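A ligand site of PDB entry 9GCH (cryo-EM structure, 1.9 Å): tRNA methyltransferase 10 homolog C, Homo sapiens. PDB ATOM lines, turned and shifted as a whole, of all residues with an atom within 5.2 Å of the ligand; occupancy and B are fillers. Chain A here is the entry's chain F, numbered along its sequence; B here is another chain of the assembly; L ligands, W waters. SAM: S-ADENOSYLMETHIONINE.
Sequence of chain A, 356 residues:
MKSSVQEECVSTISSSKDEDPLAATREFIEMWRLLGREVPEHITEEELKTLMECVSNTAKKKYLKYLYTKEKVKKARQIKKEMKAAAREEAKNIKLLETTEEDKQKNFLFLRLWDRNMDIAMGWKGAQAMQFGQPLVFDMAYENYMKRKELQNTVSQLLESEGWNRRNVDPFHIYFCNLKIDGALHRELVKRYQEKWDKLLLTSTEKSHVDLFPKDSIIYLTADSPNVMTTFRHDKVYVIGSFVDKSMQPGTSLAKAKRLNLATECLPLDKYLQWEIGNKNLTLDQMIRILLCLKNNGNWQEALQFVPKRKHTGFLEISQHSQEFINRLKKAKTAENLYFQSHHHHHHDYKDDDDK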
ATOM      1  N   TYR A 142      16.172  18.004 -16.051  1.00  0.00           N
ATOM      2  CA  TYR A 142      17.271  17.541 -15.209  1.00  0.00           C
ATOM      3  C   TYR A 142      18.085  18.696 -14.627  1.00  0.00           C
ATOM      4  O   TYR A 142      19.221  18.488 -14.216  1.00  0.00           O
ATOM      5  CB  TYR A 142      18.197  16.642 -16.023  1.00  0.00           C
ATOM      6  CG  TYR A 142      17.534  15.349 -16.459  1.00  0.00           C
ATOM      7  CD1 TYR A 142      16.822  15.274 -17.645  1.00  0.00           C
ATOM      8  CD2 TYR A 142      17.624  14.205 -15.664  1.00  0.00           C
ATOM      9  CE1 TYR A 142      16.214  14.093 -18.035  1.00  0.00           C
ATOM     10  CE2 TYR A 142      17.033  13.025 -16.051  1.00  0.00           C
ATOM     11  CZ  TYR A 142      16.320  12.974 -17.242  1.00  0.00           C
ATOM     12  OH  TYR A 142      15.725  11.810 -17.611  1.00  0.00           O
ATOM     13  N   TYR A 220      11.529   5.931 -23.962  1.00  0.00           N
ATOM     14  CA  TYR A 220      12.502   6.700 -23.210  1.00  0.00           C
ATOM     15  C   TYR A 220      13.837   5.959 -23.185  1.00  0.00           C
ATOM     16  O   TYR A 220      13.933   4.883 -22.626  1.00  0.00           O
ATOM     17  CB  TYR A 220      12.011   6.979 -21.784  1.00  0.00           C
ATOM     18  CG  TYR A 220      12.562   8.251 -21.179  1.00  0.00           C
ATOM     19  CD1 TYR A 220      11.709   9.268 -20.759  1.00  0.00           C
ATOM     20  CD2 TYR A 220      13.919   8.466 -21.073  1.00  0.00           C
ATOM     21  CE1 TYR A 220      12.195  10.443 -20.226  1.00  0.00           C
ATOM     22  CE2 TYR A 220      14.429   9.638 -20.543  1.00  0.00           C
ATOM     23  CZ  TYR A 220      13.566  10.627 -20.113  1.00  0.00           C
ATOM     24  OH  TYR A 220      14.042  11.785 -19.578  1.00  0.00           O
ATOM     25  N   LEU A 221      14.859   6.533 -23.833  1.00  0.00           N
ATOM     26  CA  LEU A 221      16.158   5.896 -23.926  1.00  0.00           C
ATOM     27  C   LEU A 221      16.929   6.134 -22.622  1.00  0.00           C
ATOM     28  O   LEU A 221      17.010   7.258 -22.136  1.00  0.00           O
ATOM     29  CB  LEU A 221      16.932   6.454 -25.113  1.00  0.00           C
ATOM     30  CG  LEU A 221      16.410   6.080 -26.496  1.00  0.00           C
ATOM     31  CD1 LEU A 221      17.118   6.888 -27.563  1.00  0.00           C
ATOM     32  CD2 LEU A 221      16.569   4.598 -26.734  1.00  0.00           C
ATOM     33  N   THR A 222      17.495   5.052 -22.084  1.00  0.00           N
ATOM     34  CA  THR A 222      18.329   5.135 -20.897  1.00  0.00           C
ATOM     35  C   THR A 222      19.154   3.863 -20.819  1.00  0.00           C
ATOM     36  O   THR A 222      18.656   2.780 -21.080  1.00  0.00           O
ATOM     37  CB  THR A 222      17.485   5.354 -19.646  1.00  0.00           C
ATOM     38  OG1 THR A 222      18.338   5.421 -18.511  1.00  0.00           O
ATOM     39  CG2 THR A 222      16.469   4.255 -19.433  1.00  0.00           C
ATOM     40  N   ALA A 223      20.434   4.009 -20.458  1.00  0.00           N
ATOM     41  CA  ALA A 223      21.334   2.869 -20.364  1.00  0.00           C
ATOM     42  C   ALA A 223      20.923   1.920 -19.238  1.00  0.00           C
ATOM     43  O   ALA A 223      21.293   0.751 -19.277  1.00  0.00           O
ATOM     44  CB  ALA A 223      22.752   3.350 -20.174  1.00  0.00           C
ATOM     45  N   ASP A 224      20.154   2.397 -18.262  1.00  0.00           N
ATOM     46  CA  ASP A 224      19.728   1.563 -17.144  1.00  0.00           C
ATOM     47  C   ASP A 224      18.500   0.729 -17.485  1.00  0.00           C
ATOM     48  O   ASP A 224      18.065  -0.068 -16.650  1.00  0.00           O
ATOM     49  CB  ASP A 224      19.440   2.416 -15.922  1.00  0.00           C
ATOM     50  CG  ASP A 224      20.632   3.246 -15.476  1.00  0.00           C
ATOM     51  OD1 ASP A 224      21.702   2.638 -15.243  1.00  0.00           O
ATOM     52  OD2 ASP A 224      20.502   4.495 -15.404  1.00  0.00           O
ATOM     53  N   VAL A 239      13.015   9.553 -26.572  1.00  0.00           N
ATOM     54  CA  VAL A 239      13.249  10.626 -25.628  1.00  0.00           C
ATOM     55  C   VAL A 239      14.651  10.446 -25.069  1.00  0.00           C
ATOM     56  O   VAL A 239      14.998   9.387 -24.573  1.00  0.00           O
ATOM     57  CB  VAL A 239      12.203  10.675 -24.506  1.00  0.00           C
ATOM     58  CG1 VAL A 239      12.419  11.862 -23.591  1.00  0.00           C
ATOM     59  CG2 VAL A 239      10.784  10.714 -25.056  1.00  0.00           C
ATOM     60  N   ILE A 240      15.440  11.522 -25.129  1.00  0.00           N
ATOM     61  CA  ILE A 240      16.792  11.534 -24.597  1.00  0.00           C
ATOM     62  C   ILE A 240      16.820  12.517 -23.433  1.00  0.00           C
ATOM     63  O   ILE A 240      16.393  13.658 -23.571  1.00  0.00           O
ATOM     64  CB  ILE A 240      17.804  11.908 -25.690  1.00  0.00           C
ATOM     65  CG1 ILE A 240      17.747  10.929 -26.858  1.00  0.00           C
ATOM     66  CG2 ILE A 240      19.209  11.985 -25.111  1.00  0.00           C
ATOM     67  CD1 ILE A 240      18.545  11.387 -28.075  1.00  0.00           C
ATOM     68  N   GLY A 241      17.370  12.063 -22.306  1.00  0.00           N
ATOM     69  CA  GLY A 241      17.527  12.932 -21.155  1.00  0.00           C
ATOM     70  C   GLY A 241      18.694  13.886 -21.308  1.00  0.00           C
ATOM     71  O   GLY A 241      19.830  13.451 -21.451  1.00  0.00           O
ATOM     72  N   SER A 242      18.412  15.189 -21.273  1.00  0.00           N
ATOM     73  CA  SER A 242      19.457  16.205 -21.323  1.00  0.00           C
ATOM     74  C   SER A 242      20.120  16.315 -19.954  1.00  0.00           C
ATOM     75  O   SER A 242      19.840  17.228 -19.176  1.00  0.00           O
ATOM     76  CB  SER A 242      18.906  17.532 -21.779  1.00  0.00           C
ATOM     77  OG  SER A 242      18.235  17.391 -23.021  1.00  0.00           O
ATOM     78  N   PHE A 243      21.004  15.356 -19.669  1.00  0.00           N
ATOM     79  CA  PHE A 243      21.522  15.163 -18.332  1.00  0.00           C
ATOM     80  C   PHE A 243      22.964  14.698 -18.427  1.00  0.00           C
ATOM     81  O   PHE A 243      23.233  13.534 -18.692  1.00  0.00           O
ATOM     82  CB  PHE A 243      20.655  14.152 -17.584  1.00  0.00           C
ATOM     83  CG  PHE A 243      21.038  13.936 -16.124  1.00  0.00           C
ATOM     84  CD1 PHE A 243      21.599  14.956 -15.379  1.00  0.00           C
ATOM     85  CD2 PHE A 243      20.813  12.709 -15.510  1.00  0.00           C
ATOM     86  CE1 PHE A 243      21.937  14.756 -14.043  1.00  0.00           C
ATOM     87  CE2 PHE A 243      21.152  12.519 -14.183  1.00  0.00           C
ATOM     88  CZ  PHE A 243      21.708  13.541 -13.446  1.00  0.00           C
ATOM     89  N   ASP A 245      25.687  13.842 -16.212  1.00  0.00           N
ATOM     90  CA  ASP A 245      25.964  13.521 -14.812  1.00  0.00           C
ATOM     91  C   ASP A 245      27.414  13.074 -14.656  1.00  0.00           C
ATOM     92  O   ASP A 245      27.700  11.880 -14.616  1.00  0.00           O
ATOM     93  CB  ASP A 245      24.981  12.487 -14.301  1.00  0.00           C
ATOM     94  CG  ASP A 245      24.988  11.199 -15.101  1.00  0.00           C
ATOM     95  OD1 ASP A 245      25.056  11.300 -16.349  1.00  0.00           O
ATOM     96  OD2 ASP A 245      24.944  10.108 -14.487  1.00  0.00           O
ATOM     97  N   GLN A 249      24.632   9.602 -11.346  1.00  0.00           N
ATOM     98  CA  GLN A 249      23.401   9.364 -10.611  1.00  0.00           C
ATOM     99  C   GLN A 249      22.603   8.313 -11.354  1.00  0.00           C
ATOM    100  O   GLN A 249      21.666   8.628 -12.083  1.00  0.00           O
ATOM    101  CB  GLN A 249      22.617  10.676 -10.488  1.00  0.00           C
ATOM    102  CG  GLN A 249      23.278  11.676  -9.544  1.00  0.00           C
ATOM    103  CD  GLN A 249      22.962  13.107  -9.885  1.00  0.00           C
ATOM    104  OE1 GLN A 249      21.803  13.525  -9.829  1.00  0.00           O
ATOM    105  NE2 GLN A 249      23.975  13.863 -10.263  1.00  0.00           N
ATOM    106  N   PRO A 250      22.959   7.018 -11.192  1.00  0.00           N
ATOM    107  CA  PRO A 250      22.280   5.953 -11.938  1.00  0.00           C
ATOM    108  C   PRO A 250      20.801   5.866 -11.576  1.00  0.00           C
ATOM    109  O   PRO A 250      20.426   6.061 -10.423  1.00  0.00           O
ATOM    110  CB  PRO A 250      23.034   4.671 -11.556  1.00  0.00           C
ATOM    111  CG  PRO A 250      24.306   5.155 -10.894  1.00  0.00           C
ATOM    112  CD  PRO A 250      23.985   6.500 -10.285  1.00  0.00           C
ATOM    113  N   GLY A 251      19.981   5.580 -12.588  1.00  0.00           N
ATOM    114  CA  GLY A 251      18.568   5.296 -12.392  1.00  0.00           C
ATOM    115  C   GLY A 251      17.695   6.549 -12.350  1.00  0.00           C
ATOM    116  O   GLY A 251      16.477   6.428 -12.286  1.00  0.00           O
ATOM    117  N   THR A 252      18.295   7.743 -12.384  1.00  0.00           N
ATOM    118  CA  THR A 252      17.514   8.973 -12.369  1.00  0.00           C
ATOM    119  C   THR A 252      16.639   9.050 -13.619  1.00  0.00           C
ATOM    120  O   THR A 252      15.463   9.386 -13.551  1.00  0.00           O
ATOM    121  CB  THR A 252      18.422  10.192 -12.257  1.00  0.00           C
ATOM    122  OG1 THR A 252      19.136  10.106 -11.020  1.00  0.00           O
ATOM    123  CG2 THR A 252      17.616  11.481 -12.270  1.00  0.00           C
ATOM    124  N   SER A 253      17.238   8.765 -14.776  1.00  0.00           N
ATOM    125  CA  SER A 253      16.538   8.804 -16.047  1.00  0.00           C
ATOM    126  C   SER A 253      15.457   7.722 -16.077  1.00  0.00           C
ATOM    127  O   SER A 253      14.344   7.972 -16.514  1.00  0.00           O
ATOM    128  CB  SER A 253      17.541   8.641 -17.162  1.00  0.00           C
ATOM    129  OG  SER A 253      17.038   9.116 -18.395  1.00  0.00           O
ATOM    130  N   LEU A 254      15.790   6.517 -15.600  1.00  0.00           N
ATOM    131  CA  LEU A 254      14.836   5.411 -15.558  1.00  0.00           C
ATOM    132  C   LEU A 254      13.671   5.727 -14.615  1.00  0.00           C
ATOM    133  O   LEU A 254      12.535   5.349 -14.886  1.00  0.00           O
ATOM    134  CB  LEU A 254      15.556   4.141 -15.140  1.00  0.00           C
ATOM    135  CG  LEU A 254      14.738   2.840 -15.160  1.00  0.00           C
ATOM    136  CD1 LEU A 254      14.355   2.449 -16.571  1.00  0.00           C
ATOM    137  CD2 LEU A 254      15.542   1.730 -14.497  1.00  0.00           C
ATOM    138  N   GLU A 265      14.196   1.806 -23.291  1.00  0.00           N
ATOM    139  CA  GLU A 265      15.099   0.972 -24.063  1.00  0.00           C
ATOM    140  C   GLU A 265      16.528   1.450 -23.820  1.00  0.00           C
ATOM    141  O   GLU A 265      16.759   2.609 -23.486  1.00  0.00           O
ATOM    142  CB  GLU A 265      14.784   0.989 -25.559  1.00  0.00           C
ATOM    143  CG  GLU A 265      13.707  -0.013 -25.965  1.00  0.00           C
ATOM    144  CD  GLU A 265      13.375   0.052 -27.450  1.00  0.00           C
ATOM    145  OE1 GLU A 265      13.864   0.970 -28.139  1.00  0.00           O
ATOM    146  OE2 GLU A 265      12.634  -0.843 -27.908  1.00  0.00           O
ATOM    147  N   CYS A 266      17.482   0.524 -23.988  1.00  0.00           N
ATOM    148  CA  CYS A 266      18.893   0.822 -23.904  1.00  0.00           C
ATOM    149  C   CYS A 266      19.574   0.382 -25.189  1.00  0.00           C
ATOM    150  O   CYS A 266      19.123  -0.534 -25.864  1.00  0.00           O
ATOM    151  CB  CYS A 266      19.535   0.180 -22.680  1.00  0.00           C
ATOM    152  SG  CYS A 266      19.589  -1.621 -22.738  1.00  0.00           S
ATOM    153  N   LEU A 267      20.670   1.057 -25.519  1.00  0.00           N
ATOM    154  CA  LEU A 267      21.464   0.677 -26.676  1.00  0.00           C
ATOM    155  C   LEU A 267      22.054  -0.708 -26.451  1.00  0.00           C
ATOM    156  O   LEU A 267      22.514  -1.027 -25.353  1.00  0.00           O
ATOM    157  CB  LEU A 267      22.568   1.696 -26.929  1.00  0.00           C
ATOM    158  CG  LEU A 267      22.123   3.057 -27.463  1.00  0.00           C
ATOM    159  CD1 LEU A 267      23.345   3.880 -27.780  1.00  0.00           C
ATOM    160  CD2 LEU A 267      21.226   2.928 -28.673  1.00  0.00           C
ATOM    161  N   LEU A 269      24.865  -2.086 -26.493  1.00  0.00           N
ATOM    162  CA  LEU A 269      26.311  -1.908 -26.463  1.00  0.00           C
ATOM    163  C   LEU A 269      27.005  -3.232 -26.176  1.00  0.00           C
ATOM    164  O   LEU A 269      28.021  -3.558 -26.804  1.00  0.00           O
ATOM    165  CB  LEU A 269      26.693  -0.857 -25.422  1.00  0.00           C
ATOM    166  CG  LEU A 269      26.062   0.523 -25.587  1.00  0.00           C
ATOM    167  CD1 LEU A 269      26.610   1.484 -24.550  1.00  0.00           C
ATOM    168  CD2 LEU A 269      26.280   1.060 -26.985  1.00  0.00           C
ATOM    169  N   LYS A 280      28.873   3.559 -19.721  1.00  0.00           N
ATOM    170  CA  LYS A 280      28.022   3.142 -20.823  1.00  0.00           C
ATOM    171  C   LYS A 280      26.959   4.195 -21.141  1.00  0.00           C
ATOM    172  O   LYS A 280      26.198   3.997 -22.081  1.00  0.00           O
ATOM    173  CB  LYS A 280      27.363   1.797 -20.531  1.00  0.00           C
ATOM    174  CG  LYS A 280      28.341   0.646 -20.547  1.00  0.00           C
ATOM    175  CD  LYS A 280      27.721  -0.714 -20.283  1.00  0.00           C
ATOM    176  CE  LYS A 280      28.727  -1.813 -20.327  1.00  0.00           C
ATOM    177  NZ  LYS A 280      28.184  -3.132 -20.002  1.00  0.00           N
ATOM    178  N   ASN A 281      26.917   5.290 -20.384  1.00  0.00           N
ATOM    179  CA  ASN A 281      26.056   6.421 -20.696  1.00  0.00           C
ATOM    180  C   ASN A 281      26.784   7.343 -21.672  1.00  0.00           C
ATOM    181  O   ASN A 281      27.689   8.073 -21.285  1.00  0.00           O
ATOM    182  CB  ASN A 281      25.650   7.151 -19.424  1.00  0.00           C
ATOM    183  CG  ASN A 281      24.834   6.301 -18.495  1.00  0.00           C
ATOM    184  OD1 ASN A 281      23.635   6.095 -18.718  1.00  0.00           O
ATOM    185  ND2 ASN A 281      25.444   5.781 -17.435  1.00  0.00           N
ATOM    186  N   LEU A 282      26.370   7.314 -22.941  1.00  0.00           N
ATOM    187  CA  LEU A 282      27.012   8.095 -23.976  1.00  0.00           C
ATOM    188  C   LEU A 282      26.537   9.539 -23.942  1.00  0.00           C
ATOM    189  O   LEU A 282      25.495   9.863 -23.382  1.00  0.00           O
ATOM    190  CB  LEU A 282      26.728   7.460 -25.345  1.00  0.00           C
ATOM    191  CG  LEU A 282      26.987   5.954 -25.434  1.00  0.00           C
ATOM    192  CD1 LEU A 282      26.739   5.470 -26.832  1.00  0.00           C
ATOM    193  CD2 LEU A 282      28.392   5.608 -24.984  1.00  0.00           C
ATOM    194  N   THR A 283      27.259  10.409 -24.641  1.00  0.00           N
ATOM    195  CA  THR A 283      26.931  11.826 -24.691  1.00  0.00           C
ATOM    196  C   THR A 283      25.749  12.049 -25.633  1.00  0.00           C
ATOM    197  O   THR A 283      25.389  11.184 -26.421  1.00  0.00           O
ATOM    198  CB  THR A 283      28.143  12.646 -25.111  1.00  0.00           C
ATOM    199  OG1 THR A 283      28.348  12.473 -26.516  1.00  0.00           O
ATOM    200  CG2 THR A 283      29.393  12.248 -24.354  1.00  0.00           C
ATOM    201  N   LEU A 284      25.166  13.258 -25.551  1.00  0.00           N
ATOM    202  CA  LEU A 284      24.009  13.595 -26.357  1.00  0.00           C
ATOM    203  C   LEU A 284      24.351  13.577 -27.850  1.00  0.00           C
ATOM    204  O   LEU A 284      23.572  13.073 -28.658  1.00  0.00           O
ATOM    205  CB  LEU A 284      23.449  14.950 -25.949  1.00  0.00           C
ATOM    206  CG  LEU A 284      22.952  15.081 -24.512  1.00  0.00           C
ATOM    207  CD1 LEU A 284      22.234  16.395 -24.307  1.00  0.00           C
ATOM    208  CD2 LEU A 284      22.022  13.953 -24.165  1.00  0.00           C
ATOM    209  N   MET A 287      24.566  10.112 -29.084  1.00  0.00           N
ATOM    210  CA  MET A 287      23.264   9.456 -29.140  1.00  0.00           C
ATOM    211  C   MET A 287      22.537   9.849 -30.441  1.00  0.00           C
ATOM    212  O   MET A 287      21.994   8.989 -31.117  1.00  0.00           O
ATOM    213  CB  MET A 287      22.418   9.815 -27.922  1.00  0.00           C
ATOM    214  CG  MET A 287      22.946   9.189 -26.637  1.00  0.00           C
ATOM    215  SD  MET A 287      22.820   7.388 -26.611  1.00  0.00           S
ATOM    216  CE  MET A 287      21.129   7.146 -27.171  1.00  0.00           C
ATOM    217  P     A B   8      35.644  13.764 -19.846  1.00  0.00           P
ATOM    218  OP1   A B   8      35.602  15.250 -19.941  1.00  0.00           O
ATOM    219  OP2   A B   8      35.302  13.118 -18.547  1.00  0.00           O
ATOM    220  O5'   A B   8      34.621  13.149 -20.922  1.00  0.00           O
ATOM    221  C5'   A B   8      34.665  13.629 -22.291  1.00  0.00           C
ATOM    222  C4'   A B   8      33.337  14.241 -22.655  1.00  0.00           C
ATOM    223  O4'   A B   8      32.273  13.327 -22.277  1.00  0.00           O
ATOM    224  C3'   A B   8      33.008  15.575 -21.972  1.00  0.00           C
ATOM    225  O3'   A B   8      32.188  16.347 -22.838  1.00  0.00           O
ATOM    226  C2'   A B   8      32.183  15.120 -20.774  1.00  0.00           C
ATOM    227  O2'   A B   8      31.363  16.150 -20.250  1.00  0.00           O
ATOM    228  C1'   A B   8      31.380  13.987 -21.416  1.00  0.00           C
ATOM    229  N9    A B   8      30.883  13.029 -20.445  1.00  0.00           N
ATOM    230  C8    A B   8      31.624  12.271 -19.564  1.00  0.00           C
ATOM    231  N7    A B   8      30.881  11.566 -18.759  1.00  0.00           N
ATOM    232  C5    A B   8      29.578  11.879 -19.125  1.00  0.00           C
ATOM    233  C6    A B   8      28.326  11.442 -18.648  1.00  0.00           C
ATOM    234  N6    A B   8      28.174  10.570 -17.645  1.00  0.00           N
ATOM    235  N1    A B   8      27.225  11.965 -19.233  1.00  0.00           N
ATOM    236  C2    A B   8      27.377  12.837 -20.236  1.00  0.00           C
ATOM    237  N3    A B   8      28.491  13.319 -20.761  1.00  0.00           N
ATOM    238  C4    A B   8      29.568  12.788 -20.164  1.00  0.00           C
HETATM  239  N   SAM L   1      23.008   8.654 -15.279  1.00  0.00           N
HETATM  240  CA  SAM L   1      22.211   9.273 -16.368  1.00  0.00           C
HETATM  241  C   SAM L   1      20.921   8.469 -16.556  1.00  0.00           C
HETATM  242  O   SAM L   1      20.573   8.219 -17.734  1.00  0.00           O
HETATM  243  OXT SAM L   1      20.323   8.118 -15.526  1.00  0.00           O
HETATM  244  CB  SAM L   1      23.017   9.295 -17.674  1.00  0.00           C
HETATM  245  CG  SAM L   1      22.641  10.410 -18.641  1.00  0.00           C
HETATM  246  SD  SAM L   1      23.158   9.949 -20.336  1.00  0.00           S
HETATM  247  CE  SAM L   1      24.853  10.499 -20.366  1.00  0.00           C
HETATM  248  C5' SAM L   1      22.341  11.235 -21.350  1.00  0.00           C
HETATM  249  C4' SAM L   1      21.129  10.641 -22.043  1.00  0.00           C
HETATM  250  O4' SAM L   1      21.545   9.882 -23.184  1.00  0.00           O
HETATM  251  C3' SAM L   1      20.381   9.664 -21.154  1.00  0.00           C
HETATM  252  O3' SAM L   1      19.467  10.389 -20.358  1.00  0.00           O
HETATM  253  C2' SAM L   1      19.749   8.720 -22.183  1.00  0.00           C
HETATM  254  O2' SAM L   1      18.516   9.268 -22.610  1.00  0.00           O
HETATM  255  C1' SAM L   1      20.771   8.709 -23.316  1.00  0.00           C
HETATM  256  N9  SAM L   1      21.668   7.564 -23.294  1.00  0.00           N
HETATM  257  C8  SAM L   1      23.002   7.600 -23.007  1.00  0.00           C
HETATM  258  N7  SAM L   1      23.585   6.439 -23.076  1.00  0.00           N
HETATM  259  C5  SAM L   1      22.578   5.574 -23.439  1.00  0.00           C
HETATM  260  C6  SAM L   1      22.581   4.188 -23.665  1.00  0.00           C
HETATM  261  N6  SAM L   1      23.662   3.432 -23.563  1.00  0.00           N
HETATM  262  N1  SAM L   1      21.414   3.610 -24.020  1.00  0.00           N
HETATM  263  C2  SAM L   1      20.331   4.379 -24.118  1.00  0.00           C
HETATM  264  N3  SAM L   1      20.220   5.699 -23.917  1.00  0.00           N
HETATM  265  C4  SAM L   1      21.385   6.242 -23.570  1.00  0.00           C
HETATM  266  O   HOH W   1      22.624   5.973 -16.046  1.00  0.00           O
HETATM  267  O   HOH W   2      21.391   6.679 -19.834  1.00  0.00           O
HETATM  268  O   HOH W   3      18.550   6.018 -15.754  1.00  0.00           O
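N9 of the ligand sits close to SD of Met 287 (3.5 Å).
Merely in contact with the ligand: Ala 223, Asp 224, Ile 240, Phe 243, Gly 251, Thr 252, Cys 266, Leu 269, Asn 281, Leu 284 and A 8 of chain B.
Hydrophobic or aromatic side chains that line the ligand: Leu 221, Ala 223, Ile 240, Phe 243, Leu 267, Leu 269, Leu 284 and Met 287.
Of the 29 residues printed, 21 come within 4 Å of the ligand.
The side-chain carboxylate of Asp 245 is in salt-bridge range of a nitrogen (N) of the ligand, at 2.5 Å.
O of Leu 221 is in hydrogen-bond range of O2' of the ligand, at 2.6 Å.
N of Leu 282 sits at hydrogen-bond distance from N7 of the ligand (2.9 Å).
The backbone carbonyl oxygen (O) of Lys 280 lies within hydrogen-bond range of a nitrogen (N6) of the ligand (3.0 Å).
The backbone NH (N) of Gly 241 sits at hydrogen-bond distance from an oxygen (O2') of the ligand (3.0 Å).
O of Gly 241 sits close to O3' of the ligand.
The backbone NH (N) of Leu 267 lies within hydrogen-bond range of a nitrogen (N1) of the ligand (3.1 Å).
The backbone NH (N) of Ser 253 is in hydrogen-bond range of an oxygen (OXT) of the ligand (3.2 Å).
OG of Ser 253 sits at hydrogen-bond distance from O3' of the ligand (3.4 Å).
N of Thr 222 sits at hydrogen-bond distance from N3 of the ligand (3.3 Å).
O of Gln 249 is in hydrogen-bond range of N of the ligand, 3.5 Å away.
Water W2 lies within hydrogen-bond range of OD1 of Asn 281 (2.6 Å), O of the ligand (2.7 Å) and N of Ala 223 (2.9 Å).
Water W3 lies within hydrogen-bond range of the side-chain carboxylate (OD2) of Asp 224 (2.5 Å), an oxygen (OXT) of the ligand (2.8 Å), the backbone NH (N) of Leu 254 (2.8 Å), the side-chain hydroxyl (OG1) of Thr 222 (2.8 Å) and the backbone NH (N) of Ser 253 (3.2 Å).
Water W1 lies within hydrogen-bond range of the side-chain carboxylate of Asp 224 (2.7 Å), a nitrogen (N) of the ligand (2.8 Å) and the side-chain amide oxygen of Asn 281 (2.9 Å).
The backbone NH (N) of Gln 249 is in hydrogen-bond range of the side-chain carboxylate (OD2) of Asp 245, 3.2 Å away.
The backbone NH (N) of Leu 221 sits at hydrogen-bond distance from the backbone carbonyl oxygen (O) of Val 239 (3.0 Å).
OG of Ser 253 lies within hydrogen-bond range of OH of Tyr 142, 3.1 Å away.
N of Thr 222 lies within hydrogen-bond range of O of Glu 265, 2.9 Å away.
O of Gln 249 sits at hydrogen-bond distance from OG1 of Thr 252, 3.1 Å away.
The side-chain carboxylate of Asp 224 lies within hydrogen-bond range of the backbone NH of Gly 251, 3.1 Å away.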
